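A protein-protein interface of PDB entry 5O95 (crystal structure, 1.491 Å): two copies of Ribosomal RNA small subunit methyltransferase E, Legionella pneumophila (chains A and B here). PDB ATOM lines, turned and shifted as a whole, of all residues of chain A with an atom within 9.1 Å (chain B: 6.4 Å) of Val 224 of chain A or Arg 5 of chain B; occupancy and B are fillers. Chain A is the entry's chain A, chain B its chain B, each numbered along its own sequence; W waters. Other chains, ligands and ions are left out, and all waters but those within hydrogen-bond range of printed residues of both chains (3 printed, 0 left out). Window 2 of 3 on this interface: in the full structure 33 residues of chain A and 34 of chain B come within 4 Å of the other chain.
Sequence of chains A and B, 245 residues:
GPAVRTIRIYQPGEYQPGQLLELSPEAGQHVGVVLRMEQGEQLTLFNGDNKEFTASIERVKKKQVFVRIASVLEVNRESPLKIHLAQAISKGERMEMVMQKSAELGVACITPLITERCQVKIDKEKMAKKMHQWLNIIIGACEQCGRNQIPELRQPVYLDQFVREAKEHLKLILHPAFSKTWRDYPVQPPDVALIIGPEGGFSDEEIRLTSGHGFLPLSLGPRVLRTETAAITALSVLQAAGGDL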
ATOM      1  N   PRO A 198       5.337 -16.739 -26.591  1.00  0.00           N
ATOM      2  CA  PRO A 198       6.359 -16.994 -27.605  1.00  0.00           C
ATOM      3  C   PRO A 198       7.287 -15.791 -27.752  1.00  0.00           C
ATOM      4  O   PRO A 198       7.075 -14.727 -27.167  1.00  0.00           O
ATOM      5  CB  PRO A 198       5.524 -17.217 -28.868  1.00  0.00           C
ATOM      6  CG  PRO A 198       4.326 -16.303 -28.669  1.00  0.00           C
ATOM      7  CD  PRO A 198       4.055 -16.298 -27.177  1.00  0.00           C
ATOM      8  N   GLU A 199       8.340 -15.991 -28.548  1.00  0.00           N
ATOM      9  CA  GLU A 199       9.352 -14.955 -28.733  1.00  0.00           C
ATOM     10  C   GLU A 199       8.730 -13.636 -29.162  1.00  0.00           C
ATOM     11  O   GLU A 199       9.206 -12.567 -28.771  1.00  0.00           O
ATOM     12  CB  GLU A 199      10.379 -15.406 -29.774  1.00  0.00           C
ATOM     13  CG  GLU A 199      11.374 -14.323 -30.167  1.00  0.00           C
ATOM     14  CD  GLU A 199      12.334 -14.767 -31.257  1.00  0.00           C
ATOM     15  OE1 GLU A 199      12.453 -15.988 -31.493  1.00  0.00           O
ATOM     16  OE2 GLU A 199      12.969 -13.890 -31.877  1.00  0.00           O
ATOM     17  N   GLY A 200       7.653 -13.690 -29.940  1.00  0.00           N
ATOM     18  CA  GLY A 200       7.001 -12.501 -30.446  1.00  0.00           C
ATOM     19  C   GLY A 200       6.078 -11.811 -29.474  1.00  0.00           C
ATOM     20  O   GLY A 200       5.543 -10.749 -29.800  1.00  0.00           O
ATOM     21  N   LEU A 220      11.823 -10.271 -15.717  1.00  0.00           N
ATOM     22  CA  LEU A 220      12.974 -11.037 -15.276  1.00  0.00           C
ATOM     23  C   LEU A 220      14.224 -10.429 -15.893  1.00  0.00           C
ATOM     24  O   LEU A 220      14.928 -11.063 -16.670  1.00  0.00           O
ATOM     25  CB  LEU A 220      12.887 -12.491 -15.729  1.00  0.00           C
ATOM     26  CG  LEU A 220      11.768 -13.321 -15.071  1.00  0.00           C
ATOM     27  CD1 LEU A 220      11.593 -14.640 -15.797  1.00  0.00           C
ATOM     28  CD2 LEU A 220      12.087 -13.511 -13.597  1.00  0.00           C
ATOM     29  N   GLY A 221      14.478  -9.168 -15.564  1.00  0.00           N
ATOM     30  CA  GLY A 221      15.696  -8.516 -15.987  1.00  0.00           C
ATOM     31  C   GLY A 221      15.618  -7.756 -17.301  1.00  0.00           C
ATOM     32  O   GLY A 221      14.649  -7.862 -18.068  1.00  0.00           O
ATOM     33  N   PRO A 222      16.679  -7.014 -17.610  1.00  0.00           N
ATOM     34  CA  PRO A 222      16.682  -6.154 -18.797  1.00  0.00           C
ATOM     35  C   PRO A 222      17.155  -6.823 -20.078  1.00  0.00           C
ATOM     36  O   PRO A 222      17.162  -6.168 -21.129  1.00  0.00           O
ATOM     37  CB  PRO A 222      17.678  -5.055 -18.384  1.00  0.00           C
ATOM     38  CG  PRO A 222      18.695  -5.789 -17.563  1.00  0.00           C
ATOM     39  CD  PRO A 222      17.882  -6.808 -16.776  1.00  0.00           C
ATOM     40  N   ARG A 223      17.590  -8.082 -20.013  1.00  0.00           N
ATOM     41  CA  ARG A 223      18.057  -8.814 -21.174  1.00  0.00           C
ATOM     42  C   ARG A 223      16.941  -9.718 -21.694  1.00  0.00           C
ATOM     43  O   ARG A 223      16.143 -10.264 -20.917  1.00  0.00           O
ATOM     44  CB  ARG A 223      19.302  -9.638 -20.805  1.00  0.00           C
ATOM     45  CG  ARG A 223      20.463  -8.766 -20.310  1.00  0.00           C
ATOM     46  CD  ARG A 223      21.571  -9.567 -19.619  1.00  0.00           C
ATOM     47  NE  ARG A 223      21.086 -10.061 -18.348  1.00  0.00           N
ATOM     48  CZ  ARG A 223      21.031  -9.360 -17.214  1.00  0.00           C
ATOM     49  NH1 ARG A 223      21.460  -8.097 -17.162  1.00  0.00           N
ATOM     50  NH2 ARG A 223      20.501  -9.936 -16.121  1.00  0.00           N
ATOM     51  N   VAL A 224      16.859  -9.819 -23.013  1.00  0.00           N
ATOM     52  CA  VAL A 224      15.833 -10.631 -23.649  1.00  0.00           C
ATOM     53  C   VAL A 224      16.245 -12.092 -23.523  1.00  0.00           C
ATOM     54  O   VAL A 224      17.297 -12.490 -24.024  1.00  0.00           O
ATOM     55  CB  VAL A 224      15.645 -10.248 -25.120  1.00  0.00           C
ATOM     56  CG1 VAL A 224      14.616 -11.177 -25.753  1.00  0.00           C
ATOM     57  CG2 VAL A 224      15.204  -8.765 -25.240  1.00  0.00           C
ATOM     58  N   LEU A 225      15.394 -12.890 -22.896  1.00  0.00           N
ATOM     59  CA  LEU A 225      15.664 -14.307 -22.681  1.00  0.00           C
ATOM     60  C   LEU A 225      15.019 -15.116 -23.797  1.00  0.00           C
ATOM     61  O   LEU A 225      13.880 -14.853 -24.186  1.00  0.00           O
ATOM     62  CB  LEU A 225      15.088 -14.745 -21.337  1.00  0.00           C
ATOM     63  CG  LEU A 225      15.664 -14.053 -20.095  1.00  0.00           C
ATOM     64  CD1 LEU A 225      15.064 -14.592 -18.781  1.00  0.00           C
ATOM     65  CD2 LEU A 225      17.220 -14.122 -20.129  1.00  0.00           C
ATOM     66  N   ARG A 226      15.754 -16.099 -24.322  1.00  0.00           N
ATOM     67  CA  ARG A 226      15.110 -17.067 -25.197  1.00  0.00           C
ATOM     68  C   ARG A 226      13.969 -17.730 -24.432  1.00  0.00           C
ATOM     69  O   ARG A 226      14.003 -17.815 -23.209  1.00  0.00           O
ATOM     70  CB  ARG A 226      16.111 -18.142 -25.632  1.00  0.00           C
ATOM     71  CG  ARG A 226      17.155 -17.617 -26.586  1.00  0.00           C
ATOM     72  CD  ARG A 226      18.119 -18.742 -26.954  1.00  0.00           C
ATOM     73  NE  ARG A 226      19.087 -18.308 -27.960  1.00  0.00           N
ATOM     74  CZ  ARG A 226      18.872 -18.343 -29.273  1.00  0.00           C
ATOM     75  NH1 ARG A 226      17.717 -18.794 -29.744  1.00  0.00           N
ATOM     76  NH2 ARG A 226      19.809 -17.923 -30.117  1.00  0.00           N
ATOM     77  N   THR A 227      12.956 -18.192 -25.180  1.00  0.00           N
ATOM     78  CA  THR A 227      11.749 -18.765 -24.577  1.00  0.00           C
ATOM     79  C   THR A 227      12.092 -19.879 -23.596  1.00  0.00           C
ATOM     80  O   THR A 227      11.505 -19.970 -22.511  1.00  0.00           O
ATOM     81  CB  THR A 227      10.850 -19.320 -25.693  1.00  0.00           C
ATOM     82  OG1 THR A 227      10.739 -18.351 -26.741  1.00  0.00           O
ATOM     83  CG2 THR A 227       9.461 -19.607 -25.162  1.00  0.00           C
ATOM     84  N   THR A 229      15.073 -20.388 -22.053  1.00  0.00           N
ATOM     85  CA  THR A 229      15.752 -19.821 -20.900  1.00  0.00           C
ATOM     86  C   THR A 229      14.753 -19.179 -19.942  1.00  0.00           C
ATOM     87  O   THR A 229      14.914 -19.260 -18.720  1.00  0.00           O
ATOM     88  CB  THR A 229      16.734 -18.760 -21.391  1.00  0.00           C
ATOM     89  OG1 THR A 229      17.534 -19.311 -22.431  1.00  0.00           O
ATOM     90  CG2 THR A 229      17.635 -18.262 -20.234  1.00  0.00           C
ATOM     91  N   ALA A 230      13.740 -18.485 -20.476  1.00  0.00           N
ATOM     92  CA  ALA A 230      12.763 -17.817 -19.617  1.00  0.00           C
ATOM     93  C   ALA A 230      12.041 -18.811 -18.723  1.00  0.00           C
ATOM     94  O   ALA A 230      11.757 -18.518 -17.555  1.00  0.00           O
ATOM     95  CB  ALA A 230      11.760 -17.047 -20.471  1.00  0.00           C
ATOM     96  N   THR A 233      14.523 -19.828 -15.975  1.00  0.00           N
ATOM     97  CA  THR A 233      14.766 -18.730 -15.057  1.00  0.00           C
ATOM     98  C   THR A 233      13.537 -18.435 -14.213  1.00  0.00           C
ATOM     99  O   THR A 233      13.646 -18.236 -12.999  1.00  0.00           O
ATOM    100  CB  THR A 233      15.182 -17.491 -15.870  1.00  0.00           C
ATOM    101  OG1 THR A 233      16.430 -17.787 -16.507  1.00  0.00           O
ATOM    102  CG2 THR A 233      15.359 -16.282 -14.990  1.00  0.00           C
ATOM    103  N   ALA B   3       5.743  -5.646 -34.759  1.00  0.00           N
ATOM    104  CA  ALA B   3       7.028  -5.002 -35.004  1.00  0.00           C
ATOM    105  C   ALA B   3       8.165  -6.018 -34.986  1.00  0.00           C
ATOM    106  O   ALA B   3       8.273  -6.837 -34.067  1.00  0.00           O
ATOM    107  CB  ALA B   3       7.280  -3.907 -33.968  1.00  0.00           C
ATOM    108  N   VAL B   4       9.014  -5.957 -36.010  1.00  0.00           N
ATOM    109  CA  VAL B   4      10.194  -6.809 -36.099  1.00  0.00           C
ATOM    110  C   VAL B   4      11.285  -6.229 -35.210  1.00  0.00           C
ATOM    111  O   VAL B   4      11.499  -5.011 -35.178  1.00  0.00           O
ATOM    112  CB  VAL B   4      10.664  -6.905 -37.564  1.00  0.00           C
ATOM    113  CG1 VAL B   4      11.726  -7.986 -37.724  1.00  0.00           C
ATOM    114  CG2 VAL B   4       9.483  -7.150 -38.497  1.00  0.00           C
ATOM    115  N   ARG B   5      11.978  -7.097 -34.477  1.00  0.00           N
ATOM    116  CA  ARG B   5      13.086  -6.648 -33.647  1.00  0.00           C
ATOM    117  C   ARG B   5      14.340  -6.501 -34.499  1.00  0.00           C
ATOM    118  O   ARG B   5      14.646  -7.361 -35.328  1.00  0.00           O
ATOM    119  CB  ARG B   5      13.345  -7.641 -32.517  1.00  0.00           C
ATOM    120  CG  ARG B   5      14.372  -7.144 -31.522  1.00  0.00           C
ATOM    121  CD  ARG B   5      14.769  -8.235 -30.562  1.00  0.00           C
ATOM    122  NE  ARG B   5      15.888  -7.834 -29.718  1.00  0.00           N
ATOM    123  CZ  ARG B   5      16.580  -8.680 -28.968  1.00  0.00           C
ATOM    124  NH1 ARG B   5      16.263  -9.969 -28.967  1.00  0.00           N
ATOM    125  NH2 ARG B   5      17.586  -8.244 -28.224  1.00  0.00           N
ATOM    126  N   THR B   6      15.057  -5.395 -34.297  1.00  0.00           N
ATOM    127  CA  THR B   6      16.204  -5.089 -35.138  1.00  0.00           C
ATOM    128  C   THR B   6      17.321  -6.097 -34.884  1.00  0.00           C
ATOM    129  O   THR B   6      17.653  -6.401 -33.736  1.00  0.00           O
ATOM    130  CB  THR B   6      16.692  -3.655 -34.889  1.00  0.00           C
ATOM    131  OG1 THR B   6      15.610  -2.735 -35.087  1.00  0.00           O
ATOM    132  CG2 THR B   6      17.818  -3.280 -35.862  1.00  0.00           C
ATOM    133  N   ILE B   7      17.899  -6.603 -35.972  1.00  0.00           N
ATOM    134  CA  ILE B   7      19.042  -7.500 -35.895  1.00  0.00           C
ATOM    135  C   ILE B   7      20.227  -6.790 -35.251  1.00  0.00           C
ATOM    136  O   ILE B   7      20.593  -5.670 -35.642  1.00  0.00           O
ATOM    137  CB  ILE B   7      19.373  -7.993 -37.312  1.00  0.00           C
ATOM    138  CG1 ILE B   7      18.253  -8.898 -37.839  1.00  0.00           C
ATOM    139  CG2 ILE B   7      20.720  -8.690 -37.344  1.00  0.00           C
ATOM    140  CD1 ILE B   7      18.093 -10.178 -37.061  1.00  0.00           C
ATOM    141  N   ARG B   8      20.853  -7.447 -34.270  1.00  0.00           N
ATOM    142  CA  ARG B   8      22.029  -6.944 -33.576  1.00  0.00           C
ATOM    143  C   ARG B   8      23.266  -7.725 -33.999  1.00  0.00           C
ATOM    144  O   ARG B   8      23.220  -8.954 -34.116  1.00  0.00           O
ATOM    145  CB  ARG B   8      21.880  -7.088 -32.062  1.00  0.00           C
ATOM    146  CG  ARG B   8      20.905  -6.097 -31.458  1.00  0.00           C
ATOM    147  CD  ARG B   8      20.441  -6.576 -30.083  1.00  0.00           C
ATOM    148  NE  ARG B   8      21.565  -6.922 -29.221  1.00  0.00           N
ATOM    149  CZ  ARG B   8      22.354  -6.038 -28.611  1.00  0.00           C
ATOM    150  NH1 ARG B   8      22.151  -4.705 -28.754  1.00  0.00           N
ATOM    151  NH2 ARG B   8      23.357  -6.459 -27.875  1.00  0.00           N
ATOM    152  N   ARG B  77      23.172  -3.048 -20.528  1.00  0.00           N
ATOM    153  CA  ARG B  77      22.247  -4.044 -19.990  1.00  0.00           C
ATOM    154  C   ARG B  77      22.965  -5.033 -19.093  1.00  0.00           C
ATOM    155  O   ARG B  77      22.527  -6.185 -18.957  1.00  0.00           O
ATOM    156  CB  ARG B  77      21.495  -4.769 -21.103  1.00  0.00           C
ATOM    157  CG  ARG B  77      20.587  -3.856 -21.885  1.00  0.00           C
ATOM    158  CD  ARG B  77      19.747  -4.614 -22.922  1.00  0.00           C
ATOM    159  NE  ARG B  77      18.854  -3.652 -23.569  1.00  0.00           N
ATOM    160  CZ  ARG B  77      19.136  -3.064 -24.735  1.00  0.00           C
ATOM    161  NH1 ARG B  77      20.242  -3.380 -25.406  1.00  0.00           N
ATOM    162  NH2 ARG B  77      18.282  -2.160 -25.226  1.00  0.00           N
ATOM    163  N   GLU B 104      23.030 -14.929 -21.461  1.00  0.00           N
ATOM    164  CA  GLU B 104      21.682 -14.354 -21.341  1.00  0.00           C
ATOM    165  C   GLU B 104      21.376 -13.949 -19.910  1.00  0.00           C
ATOM    166  O   GLU B 104      20.671 -12.950 -19.676  1.00  0.00           O
ATOM    167  CB  GLU B 104      20.611 -15.355 -21.796  1.00  0.00           C
ATOM    168  CG  GLU B 104      20.654 -15.711 -23.255  1.00  0.00           C
ATOM    169  CD  GLU B 104      19.655 -16.814 -23.620  1.00  0.00           C
ATOM    170  OE1 GLU B 104      18.478 -16.729 -23.222  1.00  0.00           O
ATOM    171  OE2 GLU B 104      20.059 -17.767 -24.314  1.00  0.00           O
ATOM    172  N   ALA B 141      25.035 -14.933 -28.217  1.00  0.00           N
ATOM    173  CA  ALA B 141      24.029 -14.775 -27.169  1.00  0.00           C
ATOM    174  C   ALA B 141      23.879 -13.311 -26.753  1.00  0.00           C
ATOM    175  O   ALA B 141      22.771 -12.860 -26.431  1.00  0.00           O
ATOM    176  CB  ALA B 141      24.378 -15.662 -25.965  1.00  0.00           C
ATOM    177  N   CYS B 142      24.974 -12.548 -26.778  1.00  0.00           N
ATOM    178  CA  CYS B 142      24.853 -11.117 -26.516  1.00  0.00           C
ATOM    179  C   CYS B 142      24.101 -10.422 -27.634  1.00  0.00           C
ATOM    180  O   CYS B 142      23.312  -9.506 -27.371  1.00  0.00           O
ATOM    181  CB  CYS B 142      26.232 -10.474 -26.336  1.00  0.00           C
ATOM    182  SG  CYS B 142      27.084 -11.053 -24.829  1.00  0.00           S
ATOM    183  N   GLU B 143      24.332 -10.843 -28.883  1.00  0.00           N
ATOM    184  CA  GLU B 143      23.537 -10.299 -29.983  1.00  0.00           C
ATOM    185  C   GLU B 143      22.062 -10.555 -29.749  1.00  0.00           C
ATOM    186  O   GLU B 143      21.231  -9.658 -29.916  1.00  0.00           O
ATOM    187  CB  GLU B 143      23.979 -10.894 -31.318  1.00  0.00           C
ATOM    188  CG  GLU B 143      25.400 -10.490 -31.682  1.00  0.00           C
ATOM    189  CD  GLU B 143      25.950 -11.194 -32.891  1.00  0.00           C
ATOM    190  OE1 GLU B 143      25.508 -12.338 -33.199  1.00  0.00           O
ATOM    191  OE2 GLU B 143      26.869 -10.613 -33.526  1.00  0.00           O
ATOM    192  N   GLN B 144      21.713 -11.775 -29.304  1.00  0.00           N
ATOM    193  CA  GLN B 144      20.311 -12.140 -29.104  1.00  0.00           C
ATOM    194  C   GLN B 144      19.681 -11.442 -27.894  1.00  0.00           C
ATOM    195  O   GLN B 144      18.530 -11.003 -27.956  1.00  0.00           O
ATOM    196  CB  GLN B 144      20.213 -13.667 -28.943  1.00  0.00           C
ATOM    197  CG  GLN B 144      18.807 -14.188 -28.526  1.00  0.00           C
ATOM    198  CD  GLN B 144      18.540 -14.143 -27.014  1.00  0.00           C
ATOM    199  OE1 GLN B 144      19.421 -14.412 -26.202  1.00  0.00           O
ATOM    200  NE2 GLN B 144      17.324 -13.778 -26.645  1.00  0.00           N
ATOM    201  N   CYS B 145      20.408 -11.347 -26.779  1.00  0.00           N
ATOM    202  CA  CYS B 145      19.782 -10.920 -25.530  1.00  0.00           C
ATOM    203  C   CYS B 145      19.861  -9.416 -25.271  1.00  0.00           C
ATOM    204  O   CYS B 145      19.145  -8.907 -24.397  1.00  0.00           O
ATOM    205  CB  CYS B 145      20.343 -11.750 -24.352  1.00  0.00           C
ATOM    206  SG  CYS B 145      21.879 -11.183 -23.677  1.00  0.00           S
ATOM    207  N   GLY B 146      20.690  -8.691 -26.015  1.00  0.00           N
ATOM    208  CA  GLY B 146      20.777  -7.250 -25.847  1.00  0.00           C
ATOM    209  C   GLY B 146      21.954  -6.757 -25.032  1.00  0.00           C
ATOM    210  O   GLY B 146      22.114  -5.543 -24.889  1.00  0.00           O
HETATM  211  O   HOH W   1      16.465  -3.700 -21.882  1.00  0.00           O
HETATM  212  O   HOH W   2      19.049 -12.131 -17.671  1.00  0.00           O
HETATM  213  O   HOH W   3      20.998 -16.580 -26.631  1.00  0.00           O
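Of the 14 printed residues of chain A, 6 touch a printed residue of chain B. Printed residues of chain A that touch a printed residue of chain B: Pro 222, Arg 223, Val 224, Leu 225, Arg 226 and Thr 229. Hydrophobic or aromatic side chains of chain A within 4 Å of the printed part of chain B: Val 224 and Leu 225. Of the 14 printed residues of chain B, 5 touch a printed residue of chain A. Along chain B the printed residues that touch a printed residue of chain A span positions 5 to 145. Among the printed residues, 12 pairs touch across the chains.
No position is printed for both chains. Of the 12 pairs that touch across the chains among the printed residues, none has its exchanged pair printed and touching as well.
The guanidinium group (NH1) of Arg 223 of chain A is in hydrogen-bond range of the backbone carbonyl oxygen (O) of Arg 77 of chain B. The guanidinium group (NE) of Arg 223 of chain A sits at hydrogen-bond distance from the backbone carbonyl oxygen (O) of Glu 104 of chain B (3.2 Å). The backbone carbonyl oxygen (O) of Val 224 of chain A sits at hydrogen-bond distance from the side-chain amide nitrogen (NE2) of Gln 144 of chain B (2.9 Å). The backbone carbonyl oxygen (O) of Cys 145 of chain B sits at hydrogen-bond distance from the backbone NH (N) of Val 224 of chain A, at 2.8 Å. NE of Arg 226 of chain A is in salt-bridge range of OE2 of Glu 104 of chain B, 3.8 Å away. OG1 of Thr 229 of chain A is in hydrogen-bond range of OE1 of Glu 104 of chain B (2.9 Å).
Of chain B, only Arg 5 (3.8 Å), Gln 144 (2.9 Å) and Cys 145 (2.8 Å) come within 4 Å of Val 224 of chain A. Of chain A, only Val 224 (3.8 Å) comes within 4 Å of Arg 5 of chain B. No residue of chain A comes within 4 Å of Val 4 of chain B. No residue of chain A comes within 4 Å of Thr 6 of chain B. Of chain A, only Arg 223 (3.4 Å) and Val 224 (2.8 Å) come within 4 Å of Cys 145 of chain B. Printed residues of chain A within 4 Å of Glu 104 of chain B: Arg 223, Leu 225, Arg 226 and Thr 229. Of the printed residues of chain A, Gln 144 of chain B touches Val 224, Leu 225 and Arg 226. Printed residues of chain B within 4 Å of Thr 229 of chain A: Glu 104. Printed residues of chain B within 4 Å of Arg 226 of chain A: Glu 104 (3.0 Å) and Gln 144 (3.6 Å). Printed residues of chain B within 4 Å of Pro 222 of chain A: Arg 77. Arg 8 of chain B touches none of the printed residues of chain A. The nearest residue of chain B that does not touch Val 224 of chain A is Glu 104 of chain B (4.5 Å). The nearest printed residue of chain B that does not touch Pro 222 of chain A is Cys 145 of chain B (4.7 Å).
O of Thr 229 of chain A is in hydrogen-bond range of OG1 of Thr 233 of chain A, at 3.1 Å. NH1 of Arg 5 of chain B sits at hydrogen-bond distance from O of Gln 144 of chain B (2.7 Å). The guanidinium group (NH1) of Arg 77 of chain B is in hydrogen-bond range of the backbone carbonyl oxygen (O) of Gly 146 of chain B, at 2.9 Å. The backbone carbonyl oxygen (O) of Ala 141 of chain B is in hydrogen-bond range of the side-chain sulfur (SG) of Cys 145 of chain B (3.3 Å).
Water W1 bridges the backbone carbonyl oxygen of Pro 222 of chain A and the guanidinium group of Arg 77 of chain B. Water W2 bridges the backbone carbonyl oxygen of Glu 104 of chain B and the guanidinium group of Arg 223 of chain A. Water W3 lies within hydrogen-bond range of OE1 of Gln 144 of chain B (2.7 Å), OE2 of Glu 104 of chain B (2.8 Å) and NE of Arg 226 of chain A (2.9 Å).
Among the printed residues, pairs that only touch across the chains: Arg 223 of chain A with Cys 145 of chain B, Pro 222 of chain A with Arg 77 of chain B, Arg 226 of chain A with Gln 144 of chain B, Leu 225 of chain A with Glu 104 of chain B, Val 224 of chain A with Arg 5 of chain B and Leu 225 of chain A with Gln 144 of chain B.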
